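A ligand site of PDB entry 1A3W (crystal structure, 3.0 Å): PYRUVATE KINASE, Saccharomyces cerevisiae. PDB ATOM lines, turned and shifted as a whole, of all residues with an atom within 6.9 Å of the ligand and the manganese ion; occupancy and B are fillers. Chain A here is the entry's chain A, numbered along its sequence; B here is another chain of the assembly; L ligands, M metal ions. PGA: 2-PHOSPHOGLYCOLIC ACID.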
ATOM      1  N   THR A  26     -21.400  -4.177  -7.816  1.00  0.00           N
ATOM      2  CA  THR A  26     -20.650  -3.433  -8.825  1.00  0.00           C
ATOM      3  C   THR A  26     -21.492  -3.401 -10.088  1.00  0.00           C
ATOM      4  O   THR A  26     -21.777  -4.439 -10.691  1.00  0.00           O
ATOM      5  CB  THR A  26     -19.295  -4.107  -9.140  1.00  0.00           C
ATOM      6  OG1 THR A  26     -18.669  -4.533  -7.930  1.00  0.00           O
ATOM      7  CG2 THR A  26     -18.382  -3.118  -9.853  1.00  0.00           C
ATOM      8  N   ARG A  49     -21.384  -0.335  -6.050  1.00  0.00           N
ATOM      9  CA  ARG A  49     -19.955  -0.169  -6.267  1.00  0.00           C
ATOM     10  C   ARG A  49     -19.684   0.475  -7.620  1.00  0.00           C
ATOM     11  O   ARG A  49     -20.318   0.155  -8.615  1.00  0.00           O
ATOM     12  CB  ARG A  49     -19.236  -1.522  -6.208  1.00  0.00           C
ATOM     13  CG  ARG A  49     -18.149  -1.614  -5.153  1.00  0.00           C
ATOM     14  CD  ARG A  49     -16.745  -1.554  -5.768  1.00  0.00           C
ATOM     15  NE  ARG A  49     -16.580  -2.537  -6.845  1.00  0.00           N
ATOM     16  CZ  ARG A  49     -15.407  -2.964  -7.305  1.00  0.00           C
ATOM     17  NH1 ARG A  49     -14.275  -2.524  -6.783  1.00  0.00           N
ATOM     18  NH2 ARG A  49     -15.366  -3.844  -8.302  1.00  0.00           N
ATOM     19  N   ASN A  51     -16.553   0.822  -9.770  1.00  0.00           N
ATOM     20  CA  ASN A  51     -15.168   0.510 -10.062  1.00  0.00           C
ATOM     21  C   ASN A  51     -14.620   1.505 -11.069  1.00  0.00           C
ATOM     22  O   ASN A  51     -14.844   1.381 -12.272  1.00  0.00           O
ATOM     23  CB  ASN A  51     -15.062  -0.920 -10.606  1.00  0.00           C
ATOM     24  CG  ASN A  51     -13.651  -1.281 -11.031  1.00  0.00           C
ATOM     25  OD1 ASN A  51     -12.678  -0.695 -10.555  1.00  0.00           O
ATOM     26  ND2 ASN A  51     -13.531  -2.249 -11.924  1.00  0.00           N
ATOM     27  N   SER A  53     -11.830   1.741 -12.116  1.00  0.00           N
ATOM     28  CA  SER A  53     -10.647   1.159 -12.749  1.00  0.00           C
ATOM     29  C   SER A  53     -10.869   1.245 -14.248  1.00  0.00           C
ATOM     30  O   SER A  53      -9.936   1.455 -15.017  1.00  0.00           O
ATOM     31  CB  SER A  53     -10.480  -0.305 -12.325  1.00  0.00           C
ATOM     32  OG  SER A  53      -9.496  -0.427 -11.309  1.00  0.00           O
ATOM     33  N   ASP A  84     -15.227   3.191  -6.010  1.00  0.00           N
ATOM     34  CA  ASP A  84     -14.017   2.392  -5.871  1.00  0.00           C
ATOM     35  C   ASP A  84     -12.866   2.981  -6.667  1.00  0.00           C
ATOM     36  O   ASP A  84     -12.777   2.791  -7.885  1.00  0.00           O
ATOM     37  CB  ASP A  84     -14.257   0.964  -6.338  1.00  0.00           C
ATOM     38  CG  ASP A  84     -13.303  -0.016  -5.693  1.00  0.00           C
ATOM     39  OD1 ASP A  84     -12.084   0.064  -5.950  1.00  0.00           O
ATOM     40  OD2 ASP A  84     -13.771  -0.880  -4.911  1.00  0.00           O
ATOM     41  N   THR A  85     -11.983   3.698  -5.992  1.00  0.00           N
ATOM     42  CA  THR A  85     -10.841   4.301  -6.646  1.00  0.00           C
ATOM     43  C   THR A  85      -9.976   3.228  -7.294  1.00  0.00           C
ATOM     44  O   THR A  85      -9.916   2.088  -6.814  1.00  0.00           O
ATOM     45  CB  THR A  85      -9.960   5.090  -5.647  1.00  0.00           C
ATOM     46  OG1 THR A  85      -9.310   4.181  -4.749  1.00  0.00           O
ATOM     47  CG2 THR A  85     -10.807   6.064  -4.846  1.00  0.00           C
ATOM     48  N   LYS A  86      -9.340   3.580  -8.400  1.00  0.00           N
ATOM     49  CA  LYS A  86      -8.458   2.655  -9.110  1.00  0.00           C
ATOM     50  C   LYS A  86      -7.059   3.034  -8.643  1.00  0.00           C
ATOM     51  O   LYS A  86      -6.304   3.701  -9.357  1.00  0.00           O
ATOM     52  CB  LYS A  86      -8.605   2.858 -10.619  1.00  0.00           C
ATOM     53  CG  LYS A  86      -7.525   2.202 -11.476  1.00  0.00           C
ATOM     54  CD  LYS A  86      -7.297   2.988 -12.750  1.00  0.00           C
ATOM     55  CE  LYS A  86      -5.840   3.385 -12.907  1.00  0.00           C
ATOM     56  NZ  LYS A  86      -5.567   4.753 -12.383  1.00  0.00           N
ATOM     57  N   GLU A  89      -2.261   0.736  -9.384  1.00  0.00           N
ATOM     58  CA  GLU A  89      -2.154  -0.589  -9.982  1.00  0.00           C
ATOM     59  C   GLU A  89      -1.301  -0.582 -11.247  1.00  0.00           C
ATOM     60  O   GLU A  89      -1.230   0.428 -11.954  1.00  0.00           O
ATOM     61  CB  GLU A  89      -3.538  -1.163 -10.297  1.00  0.00           C
ATOM     62  CG  GLU A  89      -4.166  -0.611 -11.580  1.00  0.00           C
ATOM     63  CD  GLU A  89      -5.596  -1.079 -11.769  1.00  0.00           C
ATOM     64  OE1 GLU A  89      -6.158  -1.723 -10.859  1.00  0.00           O
ATOM     65  OE2 GLU A  89      -6.162  -0.796 -12.852  1.00  0.00           O
ATOM     66  N   ARG A  91      -0.311  -2.395 -15.026  1.00  0.00           N
ATOM     67  CA  ARG A  91      -1.017  -3.080 -16.106  1.00  0.00           C
ATOM     68  C   ARG A  91      -0.139  -3.256 -17.344  1.00  0.00           C
ATOM     69  O   ARG A  91       0.680  -2.402 -17.660  1.00  0.00           O
ATOM     70  CB  ARG A  91      -2.295  -2.311 -16.490  1.00  0.00           C
ATOM     71  CG  ARG A  91      -3.525  -2.774 -15.721  1.00  0.00           C
ATOM     72  CD  ARG A  91      -4.817  -2.453 -16.460  1.00  0.00           C
ATOM     73  NE  ARG A  91      -5.921  -2.231 -15.528  1.00  0.00           N
ATOM     74  CZ  ARG A  91      -6.700  -3.194 -15.041  1.00  0.00           C
ATOM     75  NH1 ARG A  91      -6.504  -4.454 -15.401  1.00  0.00           N
ATOM     76  NH2 ARG A  91      -7.675  -2.897 -14.193  1.00  0.00           N
ATOM     77  N   SER A 213      -8.364   2.129  -2.798  1.00  0.00           N
ATOM     78  CA  SER A 213      -7.687   0.927  -3.243  1.00  0.00           C
ATOM     79  C   SER A 213      -6.182   0.901  -2.994  1.00  0.00           C
ATOM     80  O   SER A 213      -5.507   1.923  -3.126  1.00  0.00           O
ATOM     81  CB  SER A 213      -7.941   0.700  -4.722  1.00  0.00           C
ATOM     82  OG  SER A 213      -8.271  -0.655  -4.970  1.00  0.00           O
ATOM     83  N   PHE A 214      -5.682  -0.278  -2.625  1.00  0.00           N
ATOM     84  CA  PHE A 214      -4.266  -0.509  -2.357  1.00  0.00           C
ATOM     85  C   PHE A 214      -3.634   0.332  -1.253  1.00  0.00           C
ATOM     86  O   PHE A 214      -2.534   0.850  -1.401  1.00  0.00           O
ATOM     87  CB  PHE A 214      -3.471  -0.339  -3.656  1.00  0.00           C
ATOM     88  CG  PHE A 214      -3.697  -1.442  -4.646  1.00  0.00           C
ATOM     89  CD1 PHE A 214      -4.725  -1.355  -5.566  1.00  0.00           C
ATOM     90  CD2 PHE A 214      -2.896  -2.581  -4.628  1.00  0.00           C
ATOM     91  CE1 PHE A 214      -4.966  -2.392  -6.460  1.00  0.00           C
ATOM     92  CE2 PHE A 214      -3.125  -3.622  -5.518  1.00  0.00           C
ATOM     93  CZ  PHE A 214      -4.158  -3.527  -6.438  1.00  0.00           C
ATOM     94  N   LYS A 240      -9.147  -0.560   1.520  1.00  0.00           N
ATOM     95  CA  LYS A 240      -9.144  -1.870   0.880  1.00  0.00           C
ATOM     96  C   LYS A 240      -7.776  -2.521   1.106  1.00  0.00           C
ATOM     97  O   LYS A 240      -6.789  -2.082   0.518  1.00  0.00           O
ATOM     98  CB  LYS A 240      -9.386  -1.726  -0.626  1.00  0.00           C
ATOM     99  CG  LYS A 240     -10.850  -1.767  -1.060  1.00  0.00           C
ATOM    100  CD  LYS A 240     -11.082  -2.774  -2.197  1.00  0.00           C
ATOM    101  CE  LYS A 240     -11.113  -2.092  -3.546  1.00  0.00           C
ATOM    102  NZ  LYS A 240     -10.251  -0.880  -3.549  1.00  0.00           N
ATOM    103  N   ILE A 241      -7.713  -3.536   1.956  1.00  0.00           N
ATOM    104  CA  ILE A 241      -6.444  -4.210   2.246  1.00  0.00           C
ATOM    105  C   ILE A 241      -6.123  -5.158   1.109  1.00  0.00           C
ATOM    106  O   ILE A 241      -6.653  -6.264   1.052  1.00  0.00           O
ATOM    107  CB  ILE A 241      -6.541  -4.984   3.555  1.00  0.00           C
ATOM    108  CG1 ILE A 241      -7.126  -4.070   4.640  1.00  0.00           C
ATOM    109  CG2 ILE A 241      -5.168  -5.469   3.983  1.00  0.00           C
ATOM    110  CD1 ILE A 241      -6.299  -2.798   4.868  1.00  0.00           C
ATOM    111  N   GLU A 242      -5.226  -4.742   0.214  1.00  0.00           N
ATOM    112  CA  GLU A 242      -4.877  -5.558  -0.961  1.00  0.00           C
ATOM    113  C   GLU A 242      -3.494  -6.189  -1.023  1.00  0.00           C
ATOM    114  O   GLU A 242      -3.313  -7.225  -1.662  1.00  0.00           O
ATOM    115  CB  GLU A 242      -5.113  -4.728  -2.232  1.00  0.00           C
ATOM    116  CG  GLU A 242      -6.537  -4.832  -2.783  1.00  0.00           C
ATOM    117  CD  GLU A 242      -7.112  -3.490  -3.183  1.00  0.00           C
ATOM    118  OE1 GLU A 242      -7.001  -2.537  -2.383  1.00  0.00           O
ATOM    119  OE2 GLU A 242      -7.684  -3.377  -4.293  1.00  0.00           O
ATOM    120  N   MET A 261     -11.821  -3.047   3.929  1.00  0.00           N
ATOM    121  CA  MET A 261     -12.404  -3.969   2.972  1.00  0.00           C
ATOM    122  C   MET A 261     -11.454  -5.102   2.667  1.00  0.00           C
ATOM    123  O   MET A 261     -10.355  -4.884   2.157  1.00  0.00           O
ATOM    124  CB  MET A 261     -12.748  -3.254   1.676  1.00  0.00           C
ATOM    125  CG  MET A 261     -13.861  -3.918   0.904  1.00  0.00           C
ATOM    126  SD  MET A 261     -13.426  -4.177  -0.813  1.00  0.00           S
ATOM    127  CE  MET A 261     -14.729  -3.242  -1.603  1.00  0.00           C
ATOM    128  N   VAL A 262     -11.885  -6.317   2.982  1.00  0.00           N
ATOM    129  CA  VAL A 262     -11.072  -7.498   2.719  1.00  0.00           C
ATOM    130  C   VAL A 262     -10.937  -7.650   1.208  1.00  0.00           C
ATOM    131  O   VAL A 262     -11.809  -8.207   0.539  1.00  0.00           O
ATOM    132  CB  VAL A 262     -11.724  -8.765   3.306  1.00  0.00           C
ATOM    133  CG1 VAL A 262     -10.699  -9.883   3.344  1.00  0.00           C
ATOM    134  CG2 VAL A 262     -12.255  -8.486   4.699  1.00  0.00           C
ATOM    135  N   ALA A 263      -9.828  -7.132   0.688  1.00  0.00           N
ATOM    136  CA  ALA A 263      -9.537  -7.150  -0.740  1.00  0.00           C
ATOM    137  C   ALA A 263      -8.981  -8.496  -1.177  1.00  0.00           C
ATOM    138  O   ALA A 263      -7.856  -8.567  -1.682  1.00  0.00           O
ATOM    139  CB  ALA A 263      -8.559  -6.034  -1.078  1.00  0.00           C
ATOM    140  N   ARG A 264      -9.754  -9.553  -1.017  1.00  0.00           N
ATOM    141  CA  ARG A 264      -9.305 -10.893  -1.387  1.00  0.00           C
ATOM    142  C   ARG A 264      -8.692 -10.945  -2.788  1.00  0.00           C
ATOM    143  O   ARG A 264      -7.514 -11.238  -2.942  1.00  0.00           O
ATOM    144  CB  ARG A 264     -10.457 -11.892  -1.296  1.00  0.00           C
ATOM    145  CG  ARG A 264     -10.571 -12.533   0.078  1.00  0.00           C
ATOM    146  CD  ARG A 264     -11.979 -12.471   0.584  1.00  0.00           C
ATOM    147  NE  ARG A 264     -12.901 -12.889  -0.464  1.00  0.00           N
ATOM    148  CZ  ARG A 264     -13.852 -13.819  -0.296  1.00  0.00           C
ATOM    149  NH1 ARG A 264     -13.995 -14.405   0.879  1.00  0.00           N
ATOM    150  NH2 ARG A 264     -14.631 -14.159  -1.312  1.00  0.00           N
ATOM    151  N   GLY A 265      -9.497 -10.654  -3.803  1.00  0.00           N
ATOM    152  CA  GLY A 265      -9.032 -10.680  -5.182  1.00  0.00           C
ATOM    153  C   GLY A 265      -7.553 -10.449  -5.420  1.00  0.00           C
ATOM    154  O   GLY A 265      -6.878 -11.296  -6.012  1.00  0.00           O
ATOM    155  N   ASP A 266      -7.054  -9.300  -5.002  1.00  0.00           N
ATOM    156  CA  ASP A 266      -5.646  -8.969  -5.182  1.00  0.00           C
ATOM    157  C   ASP A 266      -4.860  -9.415  -3.953  1.00  0.00           C
ATOM    158  O   ASP A 266      -3.625  -9.538  -4.004  1.00  0.00           O
ATOM    159  CB  ASP A 266      -5.462  -7.468  -5.407  1.00  0.00           C
ATOM    160  CG  ASP A 266      -5.781  -7.049  -6.833  1.00  0.00           C
ATOM    161  OD1 ASP A 266      -5.104  -7.557  -7.750  1.00  0.00           O
ATOM    162  OD2 ASP A 266      -6.681  -6.202  -7.020  1.00  0.00           O
ATOM    163  N   LEU A 267      -5.556  -9.627  -2.853  1.00  0.00           N
ATOM    164  CA  LEU A 267      -4.914 -10.103  -1.636  1.00  0.00           C
ATOM    165  C   LEU A 267      -4.306 -11.459  -1.944  1.00  0.00           C
ATOM    166  O   LEU A 267      -3.089 -11.656  -1.829  1.00  0.00           O
ATOM    167  CB  LEU A 267      -5.945 -10.239  -0.517  1.00  0.00           C
ATOM    168  CG  LEU A 267      -5.349 -10.358   0.889  1.00  0.00           C
ATOM    169  CD1 LEU A 267      -4.269  -9.297   1.046  1.00  0.00           C
ATOM    170  CD2 LEU A 267      -6.424 -10.195   1.953  1.00  0.00           C
ATOM    171  N   ALA A 297     -15.122  -9.099  -0.020  1.00  0.00           N
ATOM    172  CA  ALA A 297     -15.420  -9.056  -1.450  1.00  0.00           C
ATOM    173  C   ALA A 297     -14.569  -9.916  -2.391  1.00  0.00           C
ATOM    174  O   ALA A 297     -13.556 -10.485  -1.998  1.00  0.00           O
ATOM    175  CB  ALA A 297     -15.391  -7.615  -1.918  1.00  0.00           C
ATOM    176  N   THR A 298     -15.024  -9.985  -3.645  1.00  0.00           N
ATOM    177  CA  THR A 298     -14.370 -10.703  -4.726  1.00  0.00           C
ATOM    178  C   THR A 298     -14.604 -12.215  -4.823  1.00  0.00           C
ATOM    179  O   THR A 298     -14.271 -12.967  -3.914  1.00  0.00           O
ATOM    180  CB  THR A 298     -12.847 -10.446  -4.719  1.00  0.00           C
ATOM    181  OG1 THR A 298     -12.598  -9.069  -4.446  1.00  0.00           O
ATOM    182  CG2 THR A 298     -12.246 -10.810  -6.069  1.00  0.00           C
ATOM    183  N   MET A 330     -20.001  -7.879  -0.888  1.00  0.00           N
ATOM    184  CA  MET A 330     -20.244  -7.339  -2.212  1.00  0.00           C
ATOM    185  C   MET A 330     -20.091  -8.323  -3.383  1.00  0.00           C
ATOM    186  O   MET A 330     -19.458  -9.373  -3.262  1.00  0.00           O
ATOM    187  CB  MET A 330     -19.347  -6.127  -2.443  1.00  0.00           C
ATOM    188  CG  MET A 330     -18.078  -6.405  -3.229  1.00  0.00           C
ATOM    189  SD  MET A 330     -16.980  -4.985  -3.166  1.00  0.00           S
ATOM    190  CE  MET A 330     -16.307  -4.943  -4.830  1.00  0.00           C
ATOM    191  N   SER A 332     -18.807  -8.482  -7.340  1.00  0.00           N
ATOM    192  CA  SER A 332     -18.006  -7.776  -8.325  1.00  0.00           C
ATOM    193  C   SER A 332     -18.525  -7.963  -9.753  1.00  0.00           C
ATOM    194  O   SER A 332     -19.646  -7.540 -10.066  1.00  0.00           O
ATOM    195  CB  SER A 332     -16.546  -8.260  -8.247  1.00  0.00           C
ATOM    196  OG  SER A 332     -15.799  -7.463  -7.347  1.00  0.00           O
ATOM    197  N   ARG B 312     -11.162 -17.091  -4.366  1.00  0.00           N
ATOM    198  CA  ARG B 312     -11.172 -16.795  -2.938  1.00  0.00           C
ATOM    199  C   ARG B 312     -12.208 -17.634  -2.201  1.00  0.00           C
ATOM    200  O   ARG B 312     -11.940 -18.159  -1.129  1.00  0.00           O
ATOM    201  CB  ARG B 312     -11.463 -15.318  -2.705  1.00  0.00           C
ATOM    202  CG  ARG B 312     -10.879 -14.384  -3.754  1.00  0.00           C
ATOM    203  CD  ARG B 312      -9.374 -14.531  -3.862  1.00  0.00           C
ATOM    204  NE  ARG B 312      -8.961 -14.812  -5.228  1.00  0.00           N
ATOM    205  CZ  ARG B 312      -7.778 -14.482  -5.735  1.00  0.00           C
ATOM    206  NH1 ARG B 312      -6.878 -13.857  -4.983  1.00  0.00           N
ATOM    207  NH2 ARG B 312      -7.483 -14.771  -6.997  1.00  0.00           N
HETATM  208  P   PGA L   1     -10.440  -4.589  -7.690  1.00  0.00           P
HETATM  209  O1P PGA L   1      -9.925  -5.449  -6.485  1.00  0.00           O
HETATM  210  O2P PGA L   1      -9.584  -3.939  -8.851  1.00  0.00           O
HETATM  211  O3P PGA L   1     -11.849  -5.163  -8.433  1.00  0.00           O
HETATM  212  O4P PGA L   1     -10.959  -3.417  -6.975  1.00  0.00           O
HETATM  213  C2  PGA L   1     -10.562  -6.147  -5.496  1.00  0.00           C
HETATM  214  C1  PGA L   1      -9.692  -6.747  -4.408  1.00  0.00           C
HETATM  215  O1  PGA L   1      -8.550  -6.453  -4.111  1.00  0.00           O
HETATM  216  O2  PGA L   1     -10.241  -7.721  -3.683  1.00  0.00           O
HETATM  217 MN    MN M   1      -8.039  -5.077  -5.540  1.00  0.00          MN
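The manganese ion is bound by O1 of the ligand (2.0 Å), OE2 of Glu 242 (2.1 Å), O1P of the ligand (2.1 Å) and OD2 of Asp 266 (2.3 Å).
N of Gly 265 sits at hydrogen-bond distance from O2 of the ligand, at 3.0 Å. N of Arg 264 is in hydrogen-bond range of O2 of the ligand, at 3.3 Å. An oxygen (O4P) of the ligand is in salt-bridge range of the guanidinium group (NH1) of Arg 49 (3.4 Å). O1 of the ligand lies close to N of Asp 266 (3.3 Å). OG1 of Thr 298 is in hydrogen-bond range of O2 of the ligand, at 2.8 Å.
The backbone carbonyl oxygen of Ala 263 sits close to an oxygen (O2) of the ligand (3.2 Å). Merely in contact with the ligand: Asp 84 (3.8 Å) and Lys 240 (3.7 Å). Hydrophobic or aromatic side chains that line the ligand: Ala 263. Of the 26 residues printed, 9 come within 4 Å of the ligand.
The side-chain carboxylate (OE1) of Glu 242 lies within salt-bridge range of the side-chain amino group (NZ) of Lys 240, at 3.8 Å. The backbone carbonyl oxygen (O) of Glu 242 lies close to the backbone NH (N) of Leu 267 (3.5 Å). The side-chain carboxylate (OE1) of Glu 242 lies within hydrogen-bond range of the backbone NH (N) of Phe 214 (2.6 Å). The backbone NH (N) of Ala 263 sits close to the backbone carbonyl oxygen (O) of Ile 241 (3.3 Å). The side-chain amino group (NZ) of Lys 240 lies within hydrogen-bond range of the side-chain hydroxyl (OG) of Ser 213 (2.4 Å). The guanidinium group (NH1) of Arg 312 of chain B lies within hydrogen-bond range of the backbone carbonyl oxygen (O) of Arg 264, 3.4 Å away. The side-chain carboxylate (OE1) of Glu 242 lies within hydrogen-bond range of the side-chain hydroxyl (OG) of Ser 213 (3.4 Å). The backbone carbonyl oxygen of Thr 298 sits at hydrogen-bond distance from the guanidinium group of Arg 264 (2.9 Å).
Within 4 Å of the manganese ion: Glu 242 and Asp 266. The nearest printed residue that does not touch the manganese ion is Phe 214 (4.2 Å).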
